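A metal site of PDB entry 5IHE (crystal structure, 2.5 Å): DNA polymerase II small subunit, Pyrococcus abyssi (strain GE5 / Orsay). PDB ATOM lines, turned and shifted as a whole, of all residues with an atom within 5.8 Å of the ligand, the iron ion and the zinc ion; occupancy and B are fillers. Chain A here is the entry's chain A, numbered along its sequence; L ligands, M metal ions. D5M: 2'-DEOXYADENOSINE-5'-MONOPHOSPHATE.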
ATOM      1  N   ASP A 216     -31.013 -19.677 -14.807  1.00  0.00           N
ATOM      2  CA  ASP A 216     -29.928 -18.742 -15.089  1.00  0.00           C
ATOM      3  C   ASP A 216     -29.683 -17.779 -13.939  1.00  0.00           C
ATOM      4  O   ASP A 216     -29.763 -16.551 -14.092  1.00  0.00           O
ATOM      5  CB  ASP A 216     -30.161 -18.048 -16.433  1.00  0.00           C
ATOM      6  CG  ASP A 216     -30.254 -19.026 -17.575  1.00  0.00           C
ATOM      7  OD1 ASP A 216     -29.236 -19.210 -18.278  1.00  0.00           O
ATOM      8  OD2 ASP A 216     -31.328 -19.649 -17.741  1.00  0.00           O
ATOM      9  N   HIS A 218     -26.766 -17.602 -12.276  1.00  0.00           N
ATOM     10  CA  HIS A 218     -25.416 -17.122 -12.560  1.00  0.00           C
ATOM     11  C   HIS A 218     -24.690 -16.583 -11.332  1.00  0.00           C
ATOM     12  O   HIS A 218     -24.067 -15.524 -11.403  1.00  0.00           O
ATOM     13  CB  HIS A 218     -25.413 -16.097 -13.721  1.00  0.00           C
ATOM     14  CG  HIS A 218     -25.657 -16.711 -15.051  1.00  0.00           C
ATOM     15  ND1 HIS A 218     -24.630 -17.199 -15.817  1.00  0.00           N
ATOM     16  CD2 HIS A 218     -26.827 -16.953 -15.685  1.00  0.00           C
ATOM     17  CE1 HIS A 218     -25.186 -17.702 -16.908  1.00  0.00           C
ATOM     18  NE2 HIS A 218     -26.510 -17.586 -16.867  1.00  0.00           N
ATOM     19  N   GLY A 259     -30.974 -24.794 -15.156  1.00  0.00           N
ATOM     20  CA  GLY A 259     -29.618 -24.494 -15.600  1.00  0.00           C
ATOM     21  C   GLY A 259     -29.027 -23.132 -15.338  1.00  0.00           C
ATOM     22  O   GLY A 259     -29.734 -22.183 -14.995  1.00  0.00           O
ATOM     23  N   ASP A 260     -27.678 -23.039 -15.560  1.00  0.00           N
ATOM     24  CA  ASP A 260     -26.775 -21.907 -15.341  1.00  0.00           C
ATOM     25  C   ASP A 260     -26.949 -21.334 -13.928  1.00  0.00           C
ATOM     26  O   ASP A 260     -27.141 -20.137 -13.734  1.00  0.00           O
ATOM     27  CB  ASP A 260     -26.890 -20.860 -16.449  1.00  0.00           C
ATOM     28  CG  ASP A 260     -26.330 -21.302 -17.781  1.00  0.00           C
ATOM     29  OD1 ASP A 260     -25.541 -22.241 -17.810  1.00  0.00           O
ATOM     30  OD2 ASP A 260     -26.705 -20.715 -18.805  1.00  0.00           O
ATOM     31  N   ILE A 267     -15.768 -19.914 -19.333  1.00  0.00           N
ATOM     32  CA  ILE A 267     -16.890 -20.134 -20.276  1.00  0.00           C
ATOM     33  C   ILE A 267     -16.665 -19.350 -21.583  1.00  0.00           C
ATOM     34  O   ILE A 267     -16.904 -19.880 -22.678  1.00  0.00           O
ATOM     35  CB  ILE A 267     -18.271 -19.865 -19.595  1.00  0.00           C
ATOM     36  CG1 ILE A 267     -18.453 -20.696 -18.293  1.00  0.00           C
ATOM     37  CG2 ILE A 267     -19.450 -20.066 -20.552  1.00  0.00           C
ATOM     38  CD1 ILE A 267     -18.284 -22.255 -18.397  1.00  0.00           C
ATOM     39  N   GLY A 305     -26.781 -26.333 -16.685  1.00  0.00           N
ATOM     40  CA  GLY A 305     -26.752 -25.495 -17.884  1.00  0.00           C
ATOM     41  C   GLY A 305     -25.360 -25.528 -18.498  1.00  0.00           C
ATOM     42  O   GLY A 305     -24.521 -26.309 -18.052  1.00  0.00           O
ATOM     43  N   ASN A 306     -25.072 -24.666 -19.485  1.00  0.00           N
ATOM     44  CA  ASN A 306     -23.753 -24.648 -20.136  1.00  0.00           C
ATOM     45  C   ASN A 306     -22.634 -23.916 -19.352  1.00  0.00           C
ATOM     46  O   ASN A 306     -21.470 -24.056 -19.710  1.00  0.00           O
ATOM     47  CB  ASN A 306     -23.844 -24.105 -21.575  1.00  0.00           C
ATOM     48  CG  ASN A 306     -24.471 -22.744 -21.682  1.00  0.00           C
ATOM     49  OD1 ASN A 306     -25.649 -22.553 -21.377  1.00  0.00           O
ATOM     50  ND2 ASN A 306     -23.694 -21.771 -22.141  1.00  0.00           N
ATOM     51  N   HIS A 307     -22.980 -23.168 -18.298  1.00  0.00           N
ATOM     52  CA  HIS A 307     -21.999 -22.449 -17.460  1.00  0.00           C
ATOM     53  C   HIS A 307     -21.594 -23.312 -16.288  1.00  0.00           C
ATOM     54  O   HIS A 307     -20.549 -23.093 -15.680  1.00  0.00           O
ATOM     55  CB  HIS A 307     -22.579 -21.120 -16.941  1.00  0.00           C
ATOM     56  CG  HIS A 307     -22.561 -20.006 -17.956  1.00  0.00           C
ATOM     57  ND1 HIS A 307     -21.851 -18.848 -17.727  1.00  0.00           N
ATOM     58  CD2 HIS A 307     -23.157 -19.931 -19.162  1.00  0.00           C
ATOM     59  CE1 HIS A 307     -22.038 -18.092 -18.802  1.00  0.00           C
ATOM     60  NE2 HIS A 307     -22.815 -18.696 -19.687  1.00  0.00           N
ATOM     61  N   HIS A 353     -32.336 -26.983 -20.542  1.00  0.00           N
ATOM     62  CA  HIS A 353     -31.686 -25.691 -20.373  1.00  0.00           C
ATOM     63  C   HIS A 353     -32.082 -24.694 -21.442  1.00  0.00           C
ATOM     64  O   HIS A 353     -32.304 -23.533 -21.127  1.00  0.00           O
ATOM     65  CB  HIS A 353     -30.173 -25.791 -20.226  1.00  0.00           C
ATOM     66  CG  HIS A 353     -29.536 -24.466 -19.940  1.00  0.00           C
ATOM     67  ND1 HIS A 353     -29.952 -23.678 -18.881  1.00  0.00           N
ATOM     68  CD2 HIS A 353     -28.572 -23.807 -20.613  1.00  0.00           C
ATOM     69  CE1 HIS A 353     -29.239 -22.576 -18.940  1.00  0.00           C
ATOM     70  NE2 HIS A 353     -28.396 -22.605 -19.971  1.00  0.00           N
ATOM     71  N   ARG A 355     -30.654 -24.814 -25.027  1.00  0.00           N
ATOM     72  CA  ARG A 355     -29.639 -24.698 -26.068  1.00  0.00           C
ATOM     73  C   ARG A 355     -30.232 -24.688 -27.471  1.00  0.00           C
ATOM     74  O   ARG A 355     -29.726 -23.977 -28.349  1.00  0.00           O
ATOM     75  CB  ARG A 355     -28.541 -25.780 -25.924  1.00  0.00           C
ATOM     76  CG  ARG A 355     -27.697 -25.727 -24.634  1.00  0.00           C
ATOM     77  CD  ARG A 355     -26.963 -24.409 -24.333  1.00  0.00           C
ATOM     78  NE  ARG A 355     -26.135 -23.917 -25.445  1.00  0.00           N
ATOM     79  CZ  ARG A 355     -24.870 -24.291 -25.674  1.00  0.00           C
ATOM     80  NH1 ARG A 355     -24.272 -25.169 -24.874  1.00  0.00           N
ATOM     81  NH2 ARG A 355     -24.217 -23.792 -26.704  1.00  0.00           N
ATOM     82  N   GLU A 358     -31.381 -21.312 -29.401  1.00  0.00           N
ATOM     83  CA  GLU A 358     -30.322 -20.664 -30.190  1.00  0.00           C
ATOM     84  C   GLU A 358     -30.282 -21.209 -31.601  1.00  0.00           C
ATOM     85  O   GLU A 358     -30.134 -20.428 -32.531  1.00  0.00           O
ATOM     86  CB  GLU A 358     -28.950 -20.842 -29.543  1.00  0.00           C
ATOM     87  CG  GLU A 358     -28.614 -19.719 -28.578  1.00  0.00           C
ATOM     88  CD  GLU A 358     -27.166 -19.546 -28.178  1.00  0.00           C
ATOM     89  OE1 GLU A 358     -26.544 -20.539 -27.761  1.00  0.00           O
ATOM     90  OE2 GLU A 358     -26.600 -18.487 -28.552  1.00  0.00           O
ATOM     91  N   HIS A 369     -34.947 -13.848 -30.195  1.00  0.00           N
ATOM     92  CA  HIS A 369     -35.153 -13.724 -28.748  1.00  0.00           C
ATOM     93  C   HIS A 369     -36.096 -12.501 -28.571  1.00  0.00           C
ATOM     94  O   HIS A 369     -36.675 -12.052 -29.567  1.00  0.00           O
ATOM     95  CB  HIS A 369     -33.820 -13.681 -27.945  1.00  0.00           C
ATOM     96  CG  HIS A 369     -33.133 -12.355 -27.847  1.00  0.00           C
ATOM     97  ND1 HIS A 369     -32.784 -11.813 -26.608  1.00  0.00           N
ATOM     98  CD2 HIS A 369     -32.699 -11.516 -28.816  1.00  0.00           C
ATOM     99  CE1 HIS A 369     -32.184 -10.655 -26.865  1.00  0.00           C
ATOM    100  NE2 HIS A 369     -32.111 -10.439 -28.178  1.00  0.00           N
ATOM    101  N   LYS A 392     -22.402 -23.786 -31.120  1.00  0.00           N
ATOM    102  CA  LYS A 392     -21.636 -23.794 -29.870  1.00  0.00           C
ATOM    103  C   LYS A 392     -22.286 -24.894 -29.006  1.00  0.00           C
ATOM    104  O   LYS A 392     -21.720 -25.279 -27.985  1.00  0.00           O
ATOM    105  CB  LYS A 392     -21.672 -22.427 -29.157  1.00  0.00           C
ATOM    106  CG  LYS A 392     -20.938 -21.300 -29.888  1.00  0.00           C
ATOM    107  CD  LYS A 392     -21.904 -20.425 -30.686  1.00  0.00           C
ATOM    108  CE  LYS A 392     -21.400 -19.019 -30.902  1.00  0.00           C
ATOM    109  NZ  LYS A 392     -22.370 -18.210 -31.676  1.00  0.00           N
ATOM    110  N   HIS A 416     -31.660 -20.520 -20.465  1.00  0.00           N
ATOM    111  CA  HIS A 416     -30.584 -20.195 -21.405  1.00  0.00           C
ATOM    112  C   HIS A 416     -30.677 -18.815 -22.069  1.00  0.00           C
ATOM    113  O   HIS A 416     -29.671 -18.124 -22.030  1.00  0.00           O
ATOM    114  CB  HIS A 416     -30.407 -21.296 -22.477  1.00  0.00           C
ATOM    115  CG  HIS A 416     -29.247 -21.085 -23.387  1.00  0.00           C
ATOM    116  ND1 HIS A 416     -27.952 -21.031 -22.907  1.00  0.00           N
ATOM    117  CD2 HIS A 416     -29.215 -20.926 -24.728  1.00  0.00           C
ATOM    118  CE1 HIS A 416     -27.174 -20.830 -23.964  1.00  0.00           C
ATOM    119  NE2 HIS A 416     -27.896 -20.762 -25.075  1.00  0.00           N
ATOM    120  N   VAL A 417     -31.794 -18.424 -22.726  1.00  0.00           N
ATOM    121  CA  VAL A 417     -31.842 -17.164 -23.492  1.00  0.00           C
ATOM    122  C   VAL A 417     -31.973 -15.866 -22.639  1.00  0.00           C
ATOM    123  O   VAL A 417     -31.751 -14.771 -23.192  1.00  0.00           O
ATOM    124  CB  VAL A 417     -32.888 -17.170 -24.634  1.00  0.00           C
ATOM    125  CG1 VAL A 417     -32.630 -18.335 -25.579  1.00  0.00           C
ATOM    126  CG2 VAL A 417     -34.312 -17.190 -24.109  1.00  0.00           C
ATOM    127  N   HIS A 418     -32.302 -15.987 -21.344  1.00  0.00           N
ATOM    128  CA  HIS A 418     -32.397 -14.876 -20.369  1.00  0.00           C
ATOM    129  C   HIS A 418     -33.581 -13.922 -20.610  1.00  0.00           C
ATOM    130  O   HIS A 418     -33.613 -12.835 -20.021  1.00  0.00           O
ATOM    131  CB  HIS A 418     -31.066 -14.090 -20.300  1.00  0.00           C
ATOM    132  CG  HIS A 418     -29.935 -14.855 -19.671  1.00  0.00           C
ATOM    133  ND1 HIS A 418     -28.828 -14.206 -19.174  1.00  0.00           N
ATOM    134  CD2 HIS A 418     -29.786 -16.177 -19.469  1.00  0.00           C
ATOM    135  CE1 HIS A 418     -28.042 -15.139 -18.683  1.00  0.00           C
ATOM    136  NE2 HIS A 418     -28.578 -16.345 -18.841  1.00  0.00           N
ATOM    137  N   THR A 435     -33.888 -15.136 -16.173  1.00  0.00           N
ATOM    138  CA  THR A 435     -32.580 -15.096 -15.502  1.00  0.00           C
ATOM    139  C   THR A 435     -32.592 -14.227 -14.228  1.00  0.00           C
ATOM    140  O   THR A 435     -33.503 -13.421 -14.026  1.00  0.00           O
ATOM    141  CB  THR A 435     -31.523 -14.521 -16.497  1.00  0.00           C
ATOM    142  OG1 THR A 435     -30.219 -14.631 -15.957  1.00  0.00           O
ATOM    143  CG2 THR A 435     -31.800 -13.067 -16.914  1.00  0.00           C
ATOM    144  N   GLN A 437     -29.602 -12.654 -13.764  1.00  0.00           N
ATOM    145  CA  GLN A 437     -28.401 -11.948 -14.208  1.00  0.00           C
ATOM    146  C   GLN A 437     -28.750 -10.776 -15.104  1.00  0.00           C
ATOM    147  O   GLN A 437     -29.378 -10.964 -16.136  1.00  0.00           O
ATOM    148  CB  GLN A 437     -27.453 -12.927 -14.930  1.00  0.00           C
ATOM    149  CG  GLN A 437     -26.178 -12.265 -15.458  1.00  0.00           C
ATOM    150  CD  GLN A 437     -25.227 -13.178 -16.184  1.00  0.00           C
ATOM    151  OE1 GLN A 437     -25.557 -13.781 -17.218  1.00  0.00           O
ATOM    152  NE2 GLN A 437     -24.016 -13.237 -15.702  1.00  0.00           N
ATOM    153  N   PHE A 442     -20.253  -8.760 -22.204  1.00  0.00           N
ATOM    154  CA  PHE A 442     -20.314  -9.697 -23.327  1.00  0.00           C
ATOM    155  C   PHE A 442     -21.681  -9.740 -23.991  1.00  0.00           C
ATOM    156  O   PHE A 442     -21.736  -9.747 -25.227  1.00  0.00           O
ATOM    157  CB  PHE A 442     -19.856 -11.091 -22.895  1.00  0.00           C
ATOM    158  CG  PHE A 442     -19.453 -11.977 -24.039  1.00  0.00           C
ATOM    159  CD1 PHE A 442     -20.345 -12.906 -24.570  1.00  0.00           C
ATOM    160  CD2 PHE A 442     -18.192 -11.868 -24.617  1.00  0.00           C
ATOM    161  CE1 PHE A 442     -19.982 -13.711 -25.651  1.00  0.00           C
ATOM    162  CE2 PHE A 442     -17.821 -12.700 -25.685  1.00  0.00           C
ATOM    163  CZ  PHE A 442     -18.728 -13.609 -26.188  1.00  0.00           C
ATOM    164  N   GLN A 443     -22.780  -9.772 -23.189  1.00  0.00           N
ATOM    165  CA  GLN A 443     -24.172  -9.771 -23.667  1.00  0.00           C
ATOM    166  C   GLN A 443     -24.458  -8.495 -24.485  1.00  0.00           C
ATOM    167  O   GLN A 443     -25.031  -8.589 -25.559  1.00  0.00           O
ATOM    168  CB  GLN A 443     -25.163  -9.931 -22.501  1.00  0.00           C
ATOM    169  CG  GLN A 443     -25.243 -11.367 -21.932  1.00  0.00           C
ATOM    170  CD  GLN A 443     -25.837 -11.476 -20.531  1.00  0.00           C
ATOM    171  OE1 GLN A 443     -26.323 -10.527 -19.926  1.00  0.00           O
ATOM    172  NE2 GLN A 443     -25.816 -12.670 -19.971  1.00  0.00           N
ATOM    173  N   VAL A 446     -22.847  -8.851 -27.968  1.00  0.00           N
ATOM    174  CA  VAL A 446     -23.527  -9.817 -28.838  1.00  0.00           C
ATOM    175  C   VAL A 446     -25.045  -9.496 -28.958  1.00  0.00           C
ATOM    176  O   VAL A 446     -25.826 -10.304 -29.481  1.00  0.00           O
ATOM    177  CB  VAL A 446     -23.230 -11.306 -28.468  1.00  0.00           C
ATOM    178  CG1 VAL A 446     -21.748 -11.626 -28.610  1.00  0.00           C
ATOM    179  CG2 VAL A 446     -23.744 -11.665 -27.069  1.00  0.00           C
ATOM    180  N   ILE A 448     -27.550  -9.161 -26.619  1.00  0.00           N
ATOM    181  CA  ILE A 448     -28.507  -9.911 -25.800  1.00  0.00           C
ATOM    182  C   ILE A 448     -29.041  -8.977 -24.705  1.00  0.00           C
ATOM    183  O   ILE A 448     -28.252  -8.429 -23.917  1.00  0.00           O
ATOM    184  CB  ILE A 448     -27.942 -11.281 -25.264  1.00  0.00           C
ATOM    185  CG1 ILE A 448     -28.206 -12.445 -26.264  1.00  0.00           C
ATOM    186  CG2 ILE A 448     -28.541 -11.674 -23.887  1.00  0.00           C
ATOM    187  CD1 ILE A 448     -27.305 -12.556 -27.438  1.00  0.00           C
HETATM  188  O5' D5M L   1     -26.712 -17.295 -22.579  1.00  0.00           O
HETATM  189  C5' D5M L   1     -27.485 -16.065 -22.475  1.00  0.00           C
HETATM  190  C4' D5M L   1     -27.822 -15.544 -23.864  1.00  0.00           C
HETATM  191  O4' D5M L   1     -26.610 -15.229 -24.566  1.00  0.00           O
HETATM  192  C3' D5M L   1     -28.623 -16.467 -24.782  1.00  0.00           C
HETATM  193  O3' D5M L   1     -29.611 -15.726 -25.503  1.00  0.00           O
HETATM  194  C2' D5M L   1     -27.567 -17.032 -25.723  1.00  0.00           C
HETATM  195  C1' D5M L   1     -26.594 -15.882 -25.832  1.00  0.00           C
HETATM  196  N9  D5M L   1     -25.208 -16.234 -26.147  1.00  0.00           N
HETATM  197  C8  D5M L   1     -24.343 -16.939 -25.344  1.00  0.00           C
HETATM  198  N7  D5M L   1     -23.121 -17.011 -25.813  1.00  0.00           N
HETATM  199  C5  D5M L   1     -23.196 -16.320 -27.019  1.00  0.00           C
HETATM  200  C6  D5M L   1     -22.227 -16.028 -27.992  1.00  0.00           C
HETATM  201  N6  D5M L   1     -20.960 -16.440 -27.929  1.00  0.00           N
HETATM  202  N1  D5M L   1     -22.620 -15.295 -29.065  1.00  0.00           N
HETATM  203  C2  D5M L   1     -23.896 -14.902 -29.148  1.00  0.00           C
HETATM  204  N3  D5M L   1     -24.902 -15.132 -28.291  1.00  0.00           N
HETATM  205  C4  D5M L   1     -24.484 -15.844 -27.238  1.00  0.00           C
HETATM  206  P   D5M L   1     -25.654 -17.834 -21.485  1.00  0.00           P
HETATM  207  O1P D5M L   1     -26.486 -18.531 -20.422  1.00  0.00           O
HETATM  208  O3P D5M L   1     -24.993 -16.635 -20.779  1.00  0.00           O
HETATM  209  O2P D5M L   1     -24.623 -18.666 -22.231  1.00  0.00           O
HETATM  210 FE    FE M   1     -27.564 -18.328 -18.680  1.00  0.00          FE
HETATM  211 ZN    ZN M   2     -27.026 -20.989 -20.860  1.00  0.00          ZN
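Five residues have an atom within 4 Å of the zinc ion: Asp 216, Asp 260, Asn 306, His 353 and His 416. Along chain A the residues within 4 Å of the zinc ion span positions 216 to 416. The nearest printed residue that does not touch the zinc ion is His 307 (4.4 Å).
A ring nitrogen (NE2) of His 307 is in hydrogen-bond range of an oxygen (O2P) of the ligand, at 3.1 Å. The backbone carbonyl oxygen (O) of Val 417 lies within hydrogen-bond range of an oxygen (O3') of the ligand (3.3 Å).
Within 4 Å of the iron ion: Asp 216, His 218, Asp 260, His 416 and His 418.
The iron ion is bound by the side-chain carboxylate of Asp 216 (1.9 Å), an oxygen (O1P) of the ligand (2.1 Å), a ring nitrogen (NE2) of His 218 (2.2 Å), a ring nitrogen (NE2) of His 418 (2.2 Å) and the side-chain carboxylate of Asp 260 (2.5 Å).
The zinc ion is bound by OD2 of Asp 260 (2.1 Å), OD1 of Asn 306 (2.1 Å), ND1 of His 416 (2.2 Å), NE2 of His 353 (2.3 Å) and O1P of the ligand (2.6 Å). The zinc ion has five donor atoms within binding distance.
N of His 416 lies within hydrogen-bond range of OD2 of Asp 216. OG1 of Thr 435 sits at hydrogen-bond distance from O of Asp 216, at 2.7 Å. N of Asp 216 is in hydrogen-bond range of O of Gly 259 (2.8 Å). The side-chain carboxylate of Asp 260 is in hydrogen-bond range of the backbone NH of His 307, at 2.8 Å. The side-chain amide nitrogen (NE2) of Gln 443 is in hydrogen-bond range of a ring nitrogen (ND1) of His 418 (3.5 Å). NE2 of His 416 is in hydrogen-bond range of OE1 of Glu 358 (3.0 Å). The backbone carbonyl oxygen of Gln 443 is in hydrogen-bond range of the backbone NH of Ile 448, 2.8 Å away. The guanidinium group (NH2) of Arg 355 lies within hydrogen-bond range of the backbone carbonyl oxygen (O) of Lys 392 (3.2 Å).
Glu 358 touches the ligand (OE2 to C2', 3.3 Å). Lys 392 touches the ligand (NZ to N1, 3.9 Å). Phe 442 touches the ligand (CE1 to N6, 3.7 Å). Val 446 touches the ligand. Ile 448 touches the ligand. Hydrophobic or aromatic side chains within 4 Å of the ligand: His 218, His 307, His 416, Val 417, His 418, Phe 442, Val 446 and Ile 448. Within 4 Å of the ligand: Asp 216, His 218, Asp 260, Asn 306, His 307, Glu 358, Lys 392, His 416, Val 417, His 418, Phe 442, Val 446 and Ile 448.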
